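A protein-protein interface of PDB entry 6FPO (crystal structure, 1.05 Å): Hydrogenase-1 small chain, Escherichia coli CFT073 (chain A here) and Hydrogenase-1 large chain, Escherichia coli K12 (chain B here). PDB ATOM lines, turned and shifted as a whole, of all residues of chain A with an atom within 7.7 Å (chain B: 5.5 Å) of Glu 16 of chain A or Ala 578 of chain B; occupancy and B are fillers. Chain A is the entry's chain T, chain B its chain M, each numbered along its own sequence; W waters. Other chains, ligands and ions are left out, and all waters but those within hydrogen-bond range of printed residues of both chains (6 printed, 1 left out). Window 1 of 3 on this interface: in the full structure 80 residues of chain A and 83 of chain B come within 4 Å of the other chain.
Printed residues of chain B within 4 Å of Glu 16 of chain A: Met 52, Arg 54 and Ala 578.
Of the printed residues of chain A, Ala 578 of chain B touches Glu 16 (3.7 Å).
Printed residues of chain A within 4 Å of Glu 28 of chain B: Cys 17 and Thr 18.
Of the printed residues of chain A, Cys 76 of chain B touches Cys 17.
Printed residues of chain B within 4 Å of Thr 18 of chain A: Glu 28.
Of the printed residues of chain B, Gln 122 of chain A touches Arg 54.
Asn 78 of chain A touches none of the printed residues of chain B.
The nearest printed residue of chain A that does not touch Ala 578 of chain B is Cys 17 of chain A (4.5 Å).
Of the 14 printed residues of chain B, 7 touch a printed residue of chain A.
Hydrophobic or aromatic side chains of chain B within 4 Å of the printed part of chain A: His 30, Met 52 and Ala 578.
Of the 25 printed residues of chain A, 8 touch a printed residue of chain B.
Hydrophobic or aromatic side chains of chain A that line the printed part of chain B: Leu 15.
Among the printed residues, 13 pairs touch across the chains.
Water W6 bridges O of Gln 122 of chain A (2.7 Å) and O of Arg 54 of chain B (2.8 Å).
Water W2 lies within hydrogen-bond range of OE1 of Glu 16 of chain A (2.8 Å), N of Gly 29 of chain B (2.8 Å) and OG1 of Thr 18 of chain A (2.8 Å).
Water W3 lies within hydrogen-bond range of a ring nitrogen (ND1) of His 30 of chain B (3.0 Å) and the side-chain sulfur (SG) of Cys 88 of chain A (3.0 Å).
Water W5 lies within hydrogen-bond range of the side-chain carboxylate of Asp 46 of chain A (3.0 Å) and the backbone carbonyl oxygen of Gly 29 of chain B (3.1 Å).
Water W4 bridges the backbone carbonyl oxygen of Gly 29 of chain B (3.1 Å) and the backbone carbonyl oxygen of Asp 46 of chain A (3.5 Å).
The backbone carbonyl oxygen of Gly 14 of chain A sits at hydrogen-bond distance from a ring nitrogen (NE2) of His 30 of chain B (2.8 Å).
OG1 of Thr 18 of chain A is in hydrogen-bond range of OE2 of Glu 28 of chain B (2.6 Å).
A ring nitrogen (NE2) of His 30 of chain B lies within hydrogen-bond range of the side-chain sulfur (SG) of Cys 88 of chain A (3.7 Å).
A ring nitrogen (NE2) of His 30 of chain B sits close to the backbone carbonyl oxygen (O) of His 13 of chain A (3.1 Å).
NH2 of Arg 54 of chain B lies within hydrogen-bond range of O of Ala 578 of chain B (3.2 Å).
The backbone NH (N) of Ala 578 of chain B is in hydrogen-bond range of the side-chain carboxylate (OE1) of Glu 28 of chain B.
N of Leu 15 of chain A lies within hydrogen-bond range of O of Asn 78 of chain A (2.8 Å).
The side-chain sulfur of Cys 576 of chain B sits close to the side-chain carboxylate of Glu 28 of chain B (3.4 Å).
OE2 of Glu 76 of chain A is in hydrogen-bond range of NE2 of His 13 of chain A, 3.3 Å away.
A ring nitrogen (NE2) of His 13 of chain A sits at hydrogen-bond distance from the side-chain hydroxyl (OG1) of Thr 21 of chain A, at 3.1 Å.
Leu 15 of chain A touches Met 52 of chain B (CD2 to CB, 3.8 Å).
CE of Met 52 of chain B touches O of Glu 16 of chain A (3.6 Å).
O of Glu 16 of chain A touches NH1 of Arg 54 of chain B, 3.8 Å away.
Glu 16 of chain A touches Ala 578 of chain B (O to CB, 3.7 Å).
Glu 28 of chain B touches Cys 17 of chain A (OE2 to O, 3.6 Å).
Arg 54 of chain B touches Cys 17 of chain A (NH1 to CB, 3.8 Å).
Ile 75 of chain B touches Cys 17 of chain A.
Cys 76 of chain B touches Cys 17 of chain A (C to O, 3.7 Å).
Arg 54 of chain B touches Gln 122 of chain A.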
ATOM      1  N   TRP A  11       3.203   0.446 -22.618  1.00  0.00           N
ATOM      2  CA  TRP A  11       2.020  -0.217 -23.156  1.00  0.00           C
ATOM      3  C   TRP A  11       2.491  -1.467 -23.889  1.00  0.00           C
ATOM      4  O   TRP A  11       3.220  -1.375 -24.866  1.00  0.00           O
ATOM      5  CB  TRP A  11       1.252   0.733 -24.070  1.00  0.00           C
ATOM      6  CG  TRP A  11      -0.104   0.293 -24.547  1.00  0.00           C
ATOM      7  CD1 TRP A  11      -0.555  -0.913 -24.871  1.00  0.00           C
ATOM      8  CD2 TRP A  11      -1.188   1.167 -24.792  1.00  0.00           C
ATOM      9  NE1 TRP A  11      -1.832  -0.875 -25.301  1.00  0.00           N
ATOM     10  CE2 TRP A  11      -2.258   0.396 -25.236  1.00  0.00           C
ATOM     11  CE3 TRP A  11      -1.363   2.551 -24.644  1.00  0.00           C
ATOM     12  CZ2 TRP A  11      -3.481   0.952 -25.619  1.00  0.00           C
ATOM     13  CZ3 TRP A  11      -2.555   3.127 -24.988  1.00  0.00           C
ATOM     14  CH2 TRP A  11      -3.615   2.324 -25.469  1.00  0.00           C
ATOM     15  N   ILE A  12       2.131  -2.631 -23.348  1.00  0.00           N
ATOM     16  CA  ILE A  12       2.488  -3.928 -23.920  1.00  0.00           C
ATOM     17  C   ILE A  12       1.281  -4.630 -24.497  1.00  0.00           C
ATOM     18  O   ILE A  12       0.132  -4.319 -24.171  1.00  0.00           O
ATOM     19  CB  ILE A  12       3.261  -4.852 -22.954  1.00  0.00           C
ATOM     20  CG1 ILE A  12       2.404  -5.266 -21.800  1.00  0.00           C
ATOM     21  CG2 ILE A  12       4.564  -4.160 -22.519  1.00  0.00           C
ATOM     22  CD1 ILE A  12       3.053  -6.291 -20.892  1.00  0.00           C
ATOM     23  N   HIS A  13       1.558  -5.519 -25.412  1.00  0.00           N
ATOM     24  CA  HIS A  13       0.546  -6.261 -26.206  1.00  0.00           C
ATOM     25  C   HIS A  13       0.754  -7.827 -26.225  1.00  0.00           C
ATOM     26  O   HIS A  13       1.849  -8.333 -26.594  1.00  0.00           O
ATOM     27  CB  HIS A  13       0.641  -5.766 -27.658  1.00  0.00           C
ATOM     28  CG  HIS A  13       0.305  -4.348 -27.854  1.00  0.00           C
ATOM     29  ND1 HIS A  13       1.160  -3.281 -27.702  1.00  0.00           N
ATOM     30  CD2 HIS A  13      -0.863  -3.853 -28.243  1.00  0.00           C
ATOM     31  CE1 HIS A  13       0.482  -2.177 -27.983  1.00  0.00           C
ATOM     32  NE2 HIS A  13      -0.717  -2.520 -28.403  1.00  0.00           N
ATOM     33  N   GLY A  14      -0.241  -8.509 -25.705  1.00  0.00           N
ATOM     34  CA  GLY A  14      -0.213  -9.948 -25.752  1.00  0.00           C
ATOM     35  C   GLY A  14      -0.945 -10.469 -26.979  1.00  0.00           C
ATOM     36  O   GLY A  14      -0.853  -9.884 -28.052  1.00  0.00           O
ATOM     37  N   LEU A  15      -1.717 -11.557 -26.810  1.00  0.00           N
ATOM     38  CA  LEU A  15      -2.640 -11.981 -27.866  1.00  0.00           C
ATOM     39  C   LEU A  15      -3.780 -10.998 -27.908  1.00  0.00           C
ATOM     40  O   LEU A  15      -4.463 -10.784 -26.890  1.00  0.00           O
ATOM     41  CB  LEU A  15      -3.198 -13.369 -27.611  1.00  0.00           C
ATOM     42  CG  LEU A  15      -2.216 -14.506 -27.756  1.00  0.00           C
ATOM     43  CD1 LEU A  15      -2.972 -15.808 -27.459  1.00  0.00           C
ATOM     44  CD2 LEU A  15      -1.549 -14.536 -29.126  1.00  0.00           C
ATOM     45  N   GLU A  16      -4.032 -10.402 -29.069  1.00  0.00           N
ATOM     46  CA  GLU A  16      -4.978  -9.302 -29.200  1.00  0.00           C
ATOM     47  C   GLU A  16      -5.227  -9.097 -30.686  1.00  0.00           C
ATOM     48  O   GLU A  16      -4.550  -9.682 -31.537  1.00  0.00           O
ATOM     49  CB  GLU A  16      -4.519  -7.988 -28.455  1.00  0.00           C
ATOM     50  CG  GLU A  16      -3.017  -7.611 -28.492  1.00  0.00           C
ATOM     51  CD  GLU A  16      -2.552  -6.815 -29.734  1.00  0.00           C
ATOM     52  OE1 GLU A  16      -1.384  -6.954 -30.278  1.00  0.00           O
ATOM     53  OE2 GLU A  16      -3.363  -5.959 -30.142  1.00  0.00           O
ATOM     54  N   CYS A  17      -6.201  -8.231 -30.952  1.00  0.00           N
ATOM     55  CA  CYS A  17      -6.493  -7.814 -32.321  1.00  0.00           C
ATOM     56  C   CYS A  17      -6.102  -6.360 -32.608  1.00  0.00           C
ATOM     57  O   CYS A  17      -6.236  -5.901 -33.730  1.00  0.00           O
ATOM     58  CB  CYS A  17      -7.992  -8.075 -32.655  1.00  0.00           C
ATOM     59  SG  CYS A  17      -9.054  -6.719 -32.214  1.00  0.00           S
ATOM     60  N   THR A  18      -5.671  -5.636 -31.567  1.00  0.00           N
ATOM     61  CA  THR A  18      -5.249  -4.251 -31.614  1.00  0.00           C
ATOM     62  C   THR A  18      -6.435  -3.238 -31.616  1.00  0.00           C
ATOM     63  O   THR A  18      -6.174  -2.021 -31.759  1.00  0.00           O
ATOM     64  CB  THR A  18      -4.216  -4.030 -32.722  1.00  0.00           C
ATOM     65  OG1 THR A  18      -3.251  -5.128 -32.628  1.00  0.00           O
ATOM     66  CG2 THR A  18      -3.457  -2.774 -32.611  1.00  0.00           C
ATOM     67  N   CYS A  19      -7.622  -3.722 -31.415  1.00  0.00           N
ATOM     68  CA  CYS A  19      -8.743  -2.799 -31.402  1.00  0.00           C
ATOM     69  C   CYS A  19      -8.657  -1.748 -30.293  1.00  0.00           C
ATOM     70  O   CYS A  19      -9.103  -0.600 -30.492  1.00  0.00           O
ATOM     71  CB  CYS A  19     -10.089  -3.531 -31.327  1.00  0.00           C
ATOM     72  SG  CYS A  19     -10.343  -4.454 -29.790  1.00  0.00           S
ATOM     73  N   CYS A  20      -8.118  -2.113 -29.142  1.00  0.00           N
ATOM     74  CA  CYS A  20      -8.051  -1.118 -28.042  1.00  0.00           C
ATOM     75  C   CYS A  20      -7.103   0.028 -28.351  1.00  0.00           C
ATOM     76  O   CYS A  20      -7.360   1.188 -28.014  1.00  0.00           O
ATOM     77  CB  CYS A  20      -7.709  -1.743 -26.701  1.00  0.00           C
ATOM     78  SG  CYS A  20      -8.698  -3.236 -26.361  1.00  0.00           S
ATOM     79  N   THR A  21      -5.977  -0.281 -28.995  1.00  0.00           N
ATOM     80  CA  THR A  21      -5.054   0.743 -29.448  1.00  0.00           C
ATOM     81  C   THR A  21      -5.705   1.660 -30.485  1.00  0.00           C
ATOM     82  O   THR A  21      -5.568   2.896 -30.451  1.00  0.00           O
ATOM     83  CB  THR A  21      -3.779   0.112 -30.075  1.00  0.00           C
ATOM     84  OG1 THR A  21      -2.986  -0.463 -29.056  1.00  0.00           O
ATOM     85  CG2 THR A  21      -2.920   1.109 -30.829  1.00  0.00           C
ATOM     86  N   ASP A  46       4.480  -1.002 -28.977  1.00  0.00           N
ATOM     87  CA  ASP A  46       4.936  -1.652 -30.218  1.00  0.00           C
ATOM     88  C   ASP A  46       4.223  -1.108 -31.472  1.00  0.00           C
ATOM     89  O   ASP A  46       4.817  -1.157 -32.545  1.00  0.00           O
ATOM     90  CB  ASP A  46       4.855  -3.205 -30.195  1.00  0.00           C
ATOM     91  CG  ASP A  46       5.946  -3.895 -29.339  1.00  0.00           C
ATOM     92  OD1 ASP A  46       6.974  -3.307 -29.023  1.00  0.00           O
ATOM     93  OD2 ASP A  46       5.758  -5.082 -28.980  1.00  0.00           O
ATOM     94  N   THR A  47       3.004  -0.577 -31.375  1.00  0.00           N
ATOM     95  CA  THR A  47       2.286  -0.133 -32.550  1.00  0.00           C
ATOM     96  C   THR A  47       2.821   1.185 -33.116  1.00  0.00           C
ATOM     97  O   THR A  47       2.737   1.395 -34.304  1.00  0.00           O
ATOM     98  CB  THR A  47       0.767   0.087 -32.186  1.00  0.00           C
ATOM     99  OG1 THR A  47       0.299  -1.042 -31.428  1.00  0.00           O
ATOM    100  CG2 THR A  47      -0.041   0.171 -33.404  1.00  0.00           C
ATOM    101  N   VAL A  75      -1.887  -2.762 -20.518  1.00  0.00           N
ATOM    102  CA  VAL A  75      -1.821  -4.046 -21.210  1.00  0.00           C
ATOM    103  C   VAL A  75      -3.031  -4.171 -22.094  1.00  0.00           C
ATOM    104  O   VAL A  75      -4.168  -3.984 -21.643  1.00  0.00           O
ATOM    105  CB  VAL A  75      -1.771  -5.234 -20.217  1.00  0.00           C
ATOM    106  CG1 VAL A  75      -1.667  -6.561 -21.016  1.00  0.00           C
ATOM    107  CG2 VAL A  75      -0.676  -5.058 -19.177  1.00  0.00           C
ATOM    108  N   GLU A  76      -2.772  -4.524 -23.357  1.00  0.00           N
ATOM    109  CA  GLU A  76      -3.807  -4.940 -24.305  1.00  0.00           C
ATOM    110  C   GLU A  76      -3.528  -6.407 -24.607  1.00  0.00           C
ATOM    111  O   GLU A  76      -2.379  -6.811 -24.739  1.00  0.00           O
ATOM    112  CB  GLU A  76      -3.770  -4.057 -25.570  1.00  0.00           C
ATOM    113  CG  GLU A  76      -4.869  -4.349 -26.564  1.00  0.00           C
ATOM    114  CD  GLU A  76      -4.849  -3.492 -27.804  1.00  0.00           C
ATOM    115  OE1 GLU A  76      -5.847  -3.676 -28.600  1.00  0.00           O
ATOM    116  OE2 GLU A  76      -3.997  -2.631 -27.848  1.00  0.00           O
ATOM    117  N   GLY A  77      -4.581  -7.197 -24.740  1.00  0.00           N
ATOM    118  CA  GLY A  77      -4.406  -8.597 -25.018  1.00  0.00           C
ATOM    119  C   GLY A  77      -4.068  -9.405 -23.770  1.00  0.00           C
ATOM    120  O   GLY A  77      -4.128  -8.935 -22.631  1.00  0.00           O
ATOM    121  N   ASN A  78      -3.730 -10.690 -23.994  1.00  0.00           N
ATOM    122  CA  ASN A  78      -3.537 -11.591 -22.905  1.00  0.00           C
ATOM    123  C   ASN A  78      -2.486 -12.661 -23.190  1.00  0.00           C
ATOM    124  O   ASN A  78      -2.115 -12.908 -24.338  1.00  0.00           O
ATOM    125  CB  ASN A  78      -4.861 -12.196 -22.448  1.00  0.00           C
ATOM    126  CG  ASN A  78      -5.670 -12.809 -23.562  1.00  0.00           C
ATOM    127  OD1 ASN A  78      -5.151 -13.449 -24.478  1.00  0.00           O
ATOM    128  ND2 ASN A  78      -7.009 -12.658 -23.476  1.00  0.00           N
ATOM    129  N   CYS A  88       2.421 -16.944 -28.097  1.00  0.00           N
ATOM    130  CA  CYS A  88       2.667 -15.508 -28.232  1.00  0.00           C
ATOM    131  C   CYS A  88       4.105 -15.270 -27.814  1.00  0.00           C
ATOM    132  O   CYS A  88       4.434 -15.444 -26.641  1.00  0.00           O
ATOM    133  CB  CYS A  88       1.723 -14.690 -27.380  1.00  0.00           C
ATOM    134  SG  CYS A  88       1.819 -12.912 -27.673  1.00  0.00           S
ATOM    135  N   PHE A  95       5.600 -14.412 -24.300  1.00  0.00           N
ATOM    136  CA  PHE A  95       5.094 -13.091 -23.896  1.00  0.00           C
ATOM    137  C   PHE A  95       4.926 -12.976 -22.381  1.00  0.00           C
ATOM    138  O   PHE A  95       5.154 -11.886 -21.836  1.00  0.00           O
ATOM    139  CB  PHE A  95       3.739 -12.835 -24.579  1.00  0.00           C
ATOM    140  CG  PHE A  95       2.981 -11.687 -23.989  1.00  0.00           C
ATOM    141  CD1 PHE A  95       3.398 -10.389 -24.215  1.00  0.00           C
ATOM    142  CD2 PHE A  95       1.897 -11.908 -23.189  1.00  0.00           C
ATOM    143  CE1 PHE A  95       2.717  -9.315 -23.618  1.00  0.00           C
ATOM    144  CE2 PHE A  95       1.213 -10.850 -22.611  1.00  0.00           C
ATOM    145  CZ  PHE A  95       1.633  -9.559 -22.821  1.00  0.00           C
ATOM    146  N   TRP A 112      -6.655  -2.854 -20.593  1.00  0.00           N
ATOM    147  CA  TRP A 112      -7.558  -2.350 -21.600  1.00  0.00           C
ATOM    148  C   TRP A 112      -8.237  -3.493 -22.312  1.00  0.00           C
ATOM    149  O   TRP A 112      -7.561  -4.395 -22.799  1.00  0.00           O
ATOM    150  CB  TRP A 112      -6.781  -1.559 -22.640  1.00  0.00           C
ATOM    151  CG  TRP A 112      -6.103  -0.320 -22.247  1.00  0.00           C
ATOM    152  CD1 TRP A 112      -4.799  -0.032 -22.490  1.00  0.00           C
ATOM    153  CD2 TRP A 112      -6.681   0.902 -21.697  1.00  0.00           C
ATOM    154  NE1 TRP A 112      -4.525   1.265 -22.122  1.00  0.00           N
ATOM    155  CE2 TRP A 112      -5.665   1.864 -21.671  1.00  0.00           C
ATOM    156  CE3 TRP A 112      -7.961   1.309 -21.311  1.00  0.00           C
ATOM    157  CZ2 TRP A 112      -5.881   3.177 -21.190  1.00  0.00           C
ATOM    158  CZ3 TRP A 112      -8.177   2.571 -20.870  1.00  0.00           C
ATOM    159  CH2 TRP A 112      -7.151   3.503 -20.802  1.00  0.00           C
ATOM    160  N   CYS A 115     -10.038  -8.514 -23.763  1.00  0.00           N
ATOM    161  CA  CYS A 115      -8.957  -9.516 -23.796  1.00  0.00           C
ATOM    162  C   CYS A 115      -8.173  -9.466 -22.497  1.00  0.00           C
ATOM    163  O   CYS A 115      -7.980 -10.510 -21.814  1.00  0.00           O
ATOM    164  CB  CYS A 115      -7.948  -9.300 -24.925  1.00  0.00           C
ATOM    165  SG  CYS A 115      -8.451  -9.661 -26.588  1.00  0.00           S
ATOM    166  N   ALA A 116      -7.686  -8.284 -22.111  1.00  0.00           N
ATOM    167  CA  ALA A 116      -6.835  -8.205 -20.929  1.00  0.00           C
ATOM    168  C   ALA A 116      -7.622  -8.409 -19.678  1.00  0.00           C
ATOM    169  O   ALA A 116      -7.104  -8.952 -18.681  1.00  0.00           O
ATOM    170  CB  ALA A 116      -6.113  -6.856 -20.909  1.00  0.00           C
ATOM    171  N   GLY A 119     -10.529 -12.247 -21.240  1.00  0.00           N
ATOM    172  CA  GLY A 119     -10.131 -13.298 -22.167  1.00  0.00           C
ATOM    173  C   GLY A 119     -10.499 -12.982 -23.625  1.00  0.00           C
ATOM    174  O   GLY A 119      -9.691 -13.176 -24.548  1.00  0.00           O
ATOM    175  N   VAL A 121     -12.145 -13.026 -27.410  1.00  0.00           N
ATOM    176  CA  VAL A 121     -12.475 -14.022 -28.415  1.00  0.00           C
ATOM    177  C   VAL A 121     -11.598 -15.282 -28.382  1.00  0.00           C
ATOM    178  O   VAL A 121     -12.077 -16.379 -28.514  1.00  0.00           O
ATOM    179  CB  VAL A 121     -12.585 -13.409 -29.840  1.00  0.00           C
ATOM    180  CG1 VAL A 121     -11.212 -13.174 -30.466  1.00  0.00           C
ATOM    181  CG2 VAL A 121     -13.481 -14.255 -30.716  1.00  0.00           C
ATOM    182  N   GLN A 122     -10.306 -15.095 -28.131  1.00  0.00           N
ATOM    183  CA  GLN A 122      -9.395 -16.245 -28.103  1.00  0.00           C
ATOM    184  C   GLN A 122      -9.694 -17.159 -26.958  1.00  0.00           C
ATOM    185  O   GLN A 122      -9.304 -18.339 -26.994  1.00  0.00           O
ATOM    186  CB  GLN A 122      -7.951 -15.780 -28.072  1.00  0.00           C
ATOM    187  CG  GLN A 122      -7.554 -14.830 -26.962  1.00  0.00           C
ATOM    188  CD  GLN A 122      -7.628 -13.397 -27.371  1.00  0.00           C
ATOM    189  OE1 GLN A 122      -8.485 -13.010 -28.189  1.00  0.00           O
ATOM    190  NE2 GLN A 122      -6.757 -12.582 -26.857  1.00  0.00           N
ATOM    191  N   GLU B  28       0.786  -4.240 -36.989  1.00  0.00           N
ATOM    192  CA  GLU B  28      -0.144  -4.850 -36.106  1.00  0.00           C
ATOM    193  C   GLU B  28       0.351  -6.252 -35.676  1.00  0.00           C
ATOM    194  O   GLU B  28       0.789  -7.025 -36.535  1.00  0.00           O
ATOM    195  CB  GLU B  28      -1.512  -4.947 -36.749  1.00  0.00           C
ATOM    196  CG  GLU B  28      -2.578  -5.441 -35.849  1.00  0.00           C
ATOM    197  CD  GLU B  28      -2.485  -6.845 -35.360  1.00  0.00           C
ATOM    198  OE1 GLU B  28      -1.992  -7.700 -36.106  1.00  0.00           O
ATOM    199  OE2 GLU B  28      -2.882  -7.146 -34.149  1.00  0.00           O
ATOM    200  N   GLY B  29       0.254  -6.553 -34.385  1.00  0.00           N
ATOM    201  CA  GLY B  29       0.556  -7.901 -33.915  1.00  0.00           C
ATOM    202  C   GLY B  29       2.011  -8.208 -33.759  1.00  0.00           C
ATOM    203  O   GLY B  29       2.847  -7.301 -33.637  1.00  0.00           O
ATOM    204  N   HIS B  30       2.352  -9.486 -33.813  1.00  0.00           N
ATOM    205  CA  HIS B  30       3.666  -9.973 -33.399  1.00  0.00           C
ATOM    206  C   HIS B  30       4.354 -10.649 -34.580  1.00  0.00           C
ATOM    207  O   HIS B  30       3.826 -11.609 -35.144  1.00  0.00           O
ATOM    208  CB  HIS B  30       3.502 -10.944 -32.271  1.00  0.00           C
ATOM    209  CG  HIS B  30       2.885 -10.304 -31.057  1.00  0.00           C
ATOM    210  ND1 HIS B  30       3.604  -9.586 -30.165  1.00  0.00           N
ATOM    211  CD2 HIS B  30       1.637 -10.369 -30.563  1.00  0.00           C
ATOM    212  CE1 HIS B  30       2.802  -9.197 -29.199  1.00  0.00           C
ATOM    213  NE2 HIS B  30       1.585  -9.621 -29.426  1.00  0.00           N
ATOM    214  N   MET B  52       2.450 -15.148 -33.163  1.00  0.00           N
ATOM    215  CA  MET B  52       1.220 -15.238 -32.394  1.00  0.00           C
ATOM    216  C   MET B  52       0.254 -16.179 -33.077  1.00  0.00           C
ATOM    217  O   MET B  52       0.293 -16.366 -34.273  1.00  0.00           O
ATOM    218  CB  MET B  52       0.567 -13.839 -32.237  1.00  0.00           C
ATOM    219  CG  MET B  52       0.098 -13.255 -33.569  1.00  0.00           C
ATOM    220  SD  MET B  52      -0.569 -11.621 -33.479  1.00  0.00           S
ATOM    221  CE  MET B  52      -2.002 -11.980 -32.451  1.00  0.00           C
ATOM    222  N   ARG B  54      -4.166 -17.431 -32.260  1.00  0.00           N
ATOM    223  CA  ARG B  54      -5.351 -17.454 -31.416  1.00  0.00           C
ATOM    224  C   ARG B  54      -6.311 -18.604 -31.720  1.00  0.00           C
ATOM    225  O   ARG B  54      -6.947 -19.144 -30.827  1.00  0.00           O
ATOM    226  CB  ARG B  54      -6.118 -16.121 -31.460  1.00  0.00           C
ATOM    227  CG  ARG B  54      -5.349 -14.995 -30.762  1.00  0.00           C
ATOM    228  CD  ARG B  54      -5.902 -13.611 -31.047  1.00  0.00           C
ATOM    229  NE  ARG B  54      -5.673 -13.296 -32.418  1.00  0.00           N
ATOM    230  CZ  ARG B  54      -6.455 -12.531 -33.173  1.00  0.00           C
ATOM    231  NH1 ARG B  54      -7.445 -11.830 -32.643  1.00  0.00           N
ATOM    232  NH2 ARG B  54      -6.262 -12.496 -34.491  1.00  0.00           N
ATOM    233  N   ILE B  75     -10.644 -11.014 -35.591  1.00  0.00           N
ATOM    234  CA  ILE B  75      -9.332 -11.328 -36.105  1.00  0.00           C
ATOM    235  C   ILE B  75      -8.424 -10.073 -36.031  1.00  0.00           C
ATOM    236  O   ILE B  75      -7.228 -10.201 -35.797  1.00  0.00           O
ATOM    237  CB  ILE B  75      -9.411 -11.938 -37.490  1.00  0.00           C
ATOM    238  CG1 ILE B  75      -9.989 -13.336 -37.423  1.00  0.00           C
ATOM    239  CG2 ILE B  75      -8.057 -11.933 -38.196  1.00  0.00           C
ATOM    240  CD1 ILE B  75     -10.331 -13.995 -38.736  1.00  0.00           C
ATOM    241  N   CYS B  76      -8.999  -8.895 -36.321  1.00  0.00           N
ATOM    242  CA  CYS B  76      -8.187  -7.727 -36.407  1.00  0.00           C
ATOM    243  C   CYS B  76      -8.963  -6.455 -36.224  1.00  0.00           C
ATOM    244  O   CYS B  76     -10.007  -6.248 -36.837  1.00  0.00           O
ATOM    245  CB  CYS B  76      -7.385  -7.747 -37.619  1.00  0.00           C
ATOM    246  SG  CYS B  76      -6.109  -6.471 -37.613  1.00  0.00           S
ATOM    247  N   CYS B 576       0.037  -7.181 -40.995  1.00  0.00           N
ATOM    248  CA  CYS B 576      -0.981  -7.360 -39.957  1.00  0.00           C
ATOM    249  C   CYS B 576      -0.869  -8.793 -39.483  1.00  0.00           C
ATOM    250  O   CYS B 576      -1.336  -9.733 -40.164  1.00  0.00           O
ATOM    251  CB  CYS B 576      -2.403  -7.109 -40.536  1.00  0.00           C
ATOM    252  SG  CYS B 576      -3.502  -6.959 -39.089  1.00  0.00           S
ATOM    253  N   LEU B 577      -0.214  -8.984 -38.353  1.00  0.00           N
ATOM    254  CA  LEU B 577       0.134 -10.333 -37.947  1.00  0.00           C
ATOM    255  C   LEU B 577      -1.004 -11.072 -37.298  1.00  0.00           C
ATOM    256  O   LEU B 577      -1.088 -12.312 -37.420  1.00  0.00           O
ATOM    257  CB  LEU B 577       1.396 -10.341 -37.089  1.00  0.00           C
ATOM    258  CG  LEU B 577       2.692 -10.282 -37.908  1.00  0.00           C
ATOM    259  CD1 LEU B 577       2.983 -11.625 -38.561  1.00  0.00           C
ATOM    260  CD2 LEU B 577       2.744  -9.200 -38.962  1.00  0.00           C
ATOM    261  N   ALA B 578      -1.913 -10.335 -36.639  1.00  0.00           N
ATOM    262  CA  ALA B 578      -3.124 -10.958 -36.089  1.00  0.00           C
ATOM    263  C   ALA B 578      -3.975 -11.488 -37.231  1.00  0.00           C
ATOM    264  O   ALA B 578      -4.498 -12.623 -37.172  1.00  0.00           O
ATOM    265  CB  ALA B 578      -3.891  -9.979 -35.211  1.00  0.00           C
ATOM    266  N   CYS B 579      -4.107 -10.695 -38.295  1.00  0.00           N
ATOM    267  CA  CYS B 579      -4.779 -11.199 -39.508  1.00  0.00           C
ATOM    268  C   CYS B 579      -4.083 -12.453 -40.001  1.00  0.00           C
ATOM    269  O   CYS B 579      -4.759 -13.398 -40.425  1.00  0.00           O
ATOM    270  CB  CYS B 579      -4.732 -10.146 -40.565  1.00  0.00           C
ATOM    271  SG  CYS B 579      -6.135  -9.023 -40.522  1.00  0.00           S
ATOM    272  N   SER B 580      -2.756 -12.440 -40.084  1.00  0.00           N
ATOM    273  CA  SER B 580      -2.063 -13.498 -40.814  1.00  0.00           C
ATOM    274  C   SER B 580      -2.275 -14.865 -40.177  1.00  0.00           C
ATOM    275  O   SER B 580      -2.236 -15.871 -40.892  1.00  0.00           O
ATOM    276  CB  SER B 580      -0.577 -13.203 -40.894  1.00  0.00           C
ATOM    277  OG  SER B 580       0.124 -13.411 -39.683  1.00  0.00           O
ATOM    278  N   THR B 581      -2.427 -14.891 -38.863  1.00  0.00           N
ATOM    279  CA  THR B 581      -2.472 -16.094 -38.055  1.00  0.00           C
ATOM    280  C   THR B 581      -3.859 -16.474 -37.594  1.00  0.00           C
ATOM    281  O   THR B 581      -4.205 -17.653 -37.510  1.00  0.00           O
ATOM    282  CB  THR B 581      -1.512 -15.897 -36.835  1.00  0.00           C
ATOM    283  OG1 THR B 581      -1.877 -14.733 -36.103  1.00  0.00           O
ATOM    284  CG2 THR B 581      -0.057 -15.861 -37.314  1.00  0.00           C
ATOM    285  N   HIS B 582      -4.660 -15.425 -37.276  1.00  0.00           N
ATOM    286  CA  HIS B 582      -6.048 -15.642 -36.821  1.00  0.00           C
ATOM    287  C   HIS B 582      -6.192 -16.825 -35.822  1.00  0.00           C
ATOM    288  O   HIS B 582      -7.104 -17.649 -35.980  1.00  0.00           O
ATOM    289  CB  HIS B 582      -7.036 -15.700 -38.008  1.00  0.00           C
ATOM    290  CG  HIS B 582      -6.561 -16.513 -39.192  1.00  0.00           C
ATOM    291  ND1 HIS B 582      -5.693 -16.012 -40.145  1.00  0.00           N
ATOM    292  CD2 HIS B 582      -6.878 -17.776 -39.605  1.00  0.00           C
ATOM    293  CE1 HIS B 582      -5.464 -16.957 -41.061  1.00  0.00           C
ATOM    294  NE2 HIS B 582      -6.178 -18.034 -40.771  1.00  0.00           N
ATOM    295  OXT HIS B 582      -5.376 -16.862 -34.843  1.00  0.00           O
HETATM  296  O   HOH W   1      -7.902 -11.009 -29.967  1.00  0.00           O
HETATM  297  O   HOH W   2      -0.458  -5.080 -32.092  1.00  0.00           O
HETATM  298  O   HOH W   3       4.435 -11.387 -27.957  1.00  0.00           O
HETATM  299  O   HOH W   4       3.676  -4.355 -33.181  1.00  0.00           O
HETATM  300  O   HOH W   5       4.917  -6.569 -31.453  1.00  0.00           O
HETATM  301  O   HOH W   6      -7.047 -19.409 -28.085  1.00  0.00           O
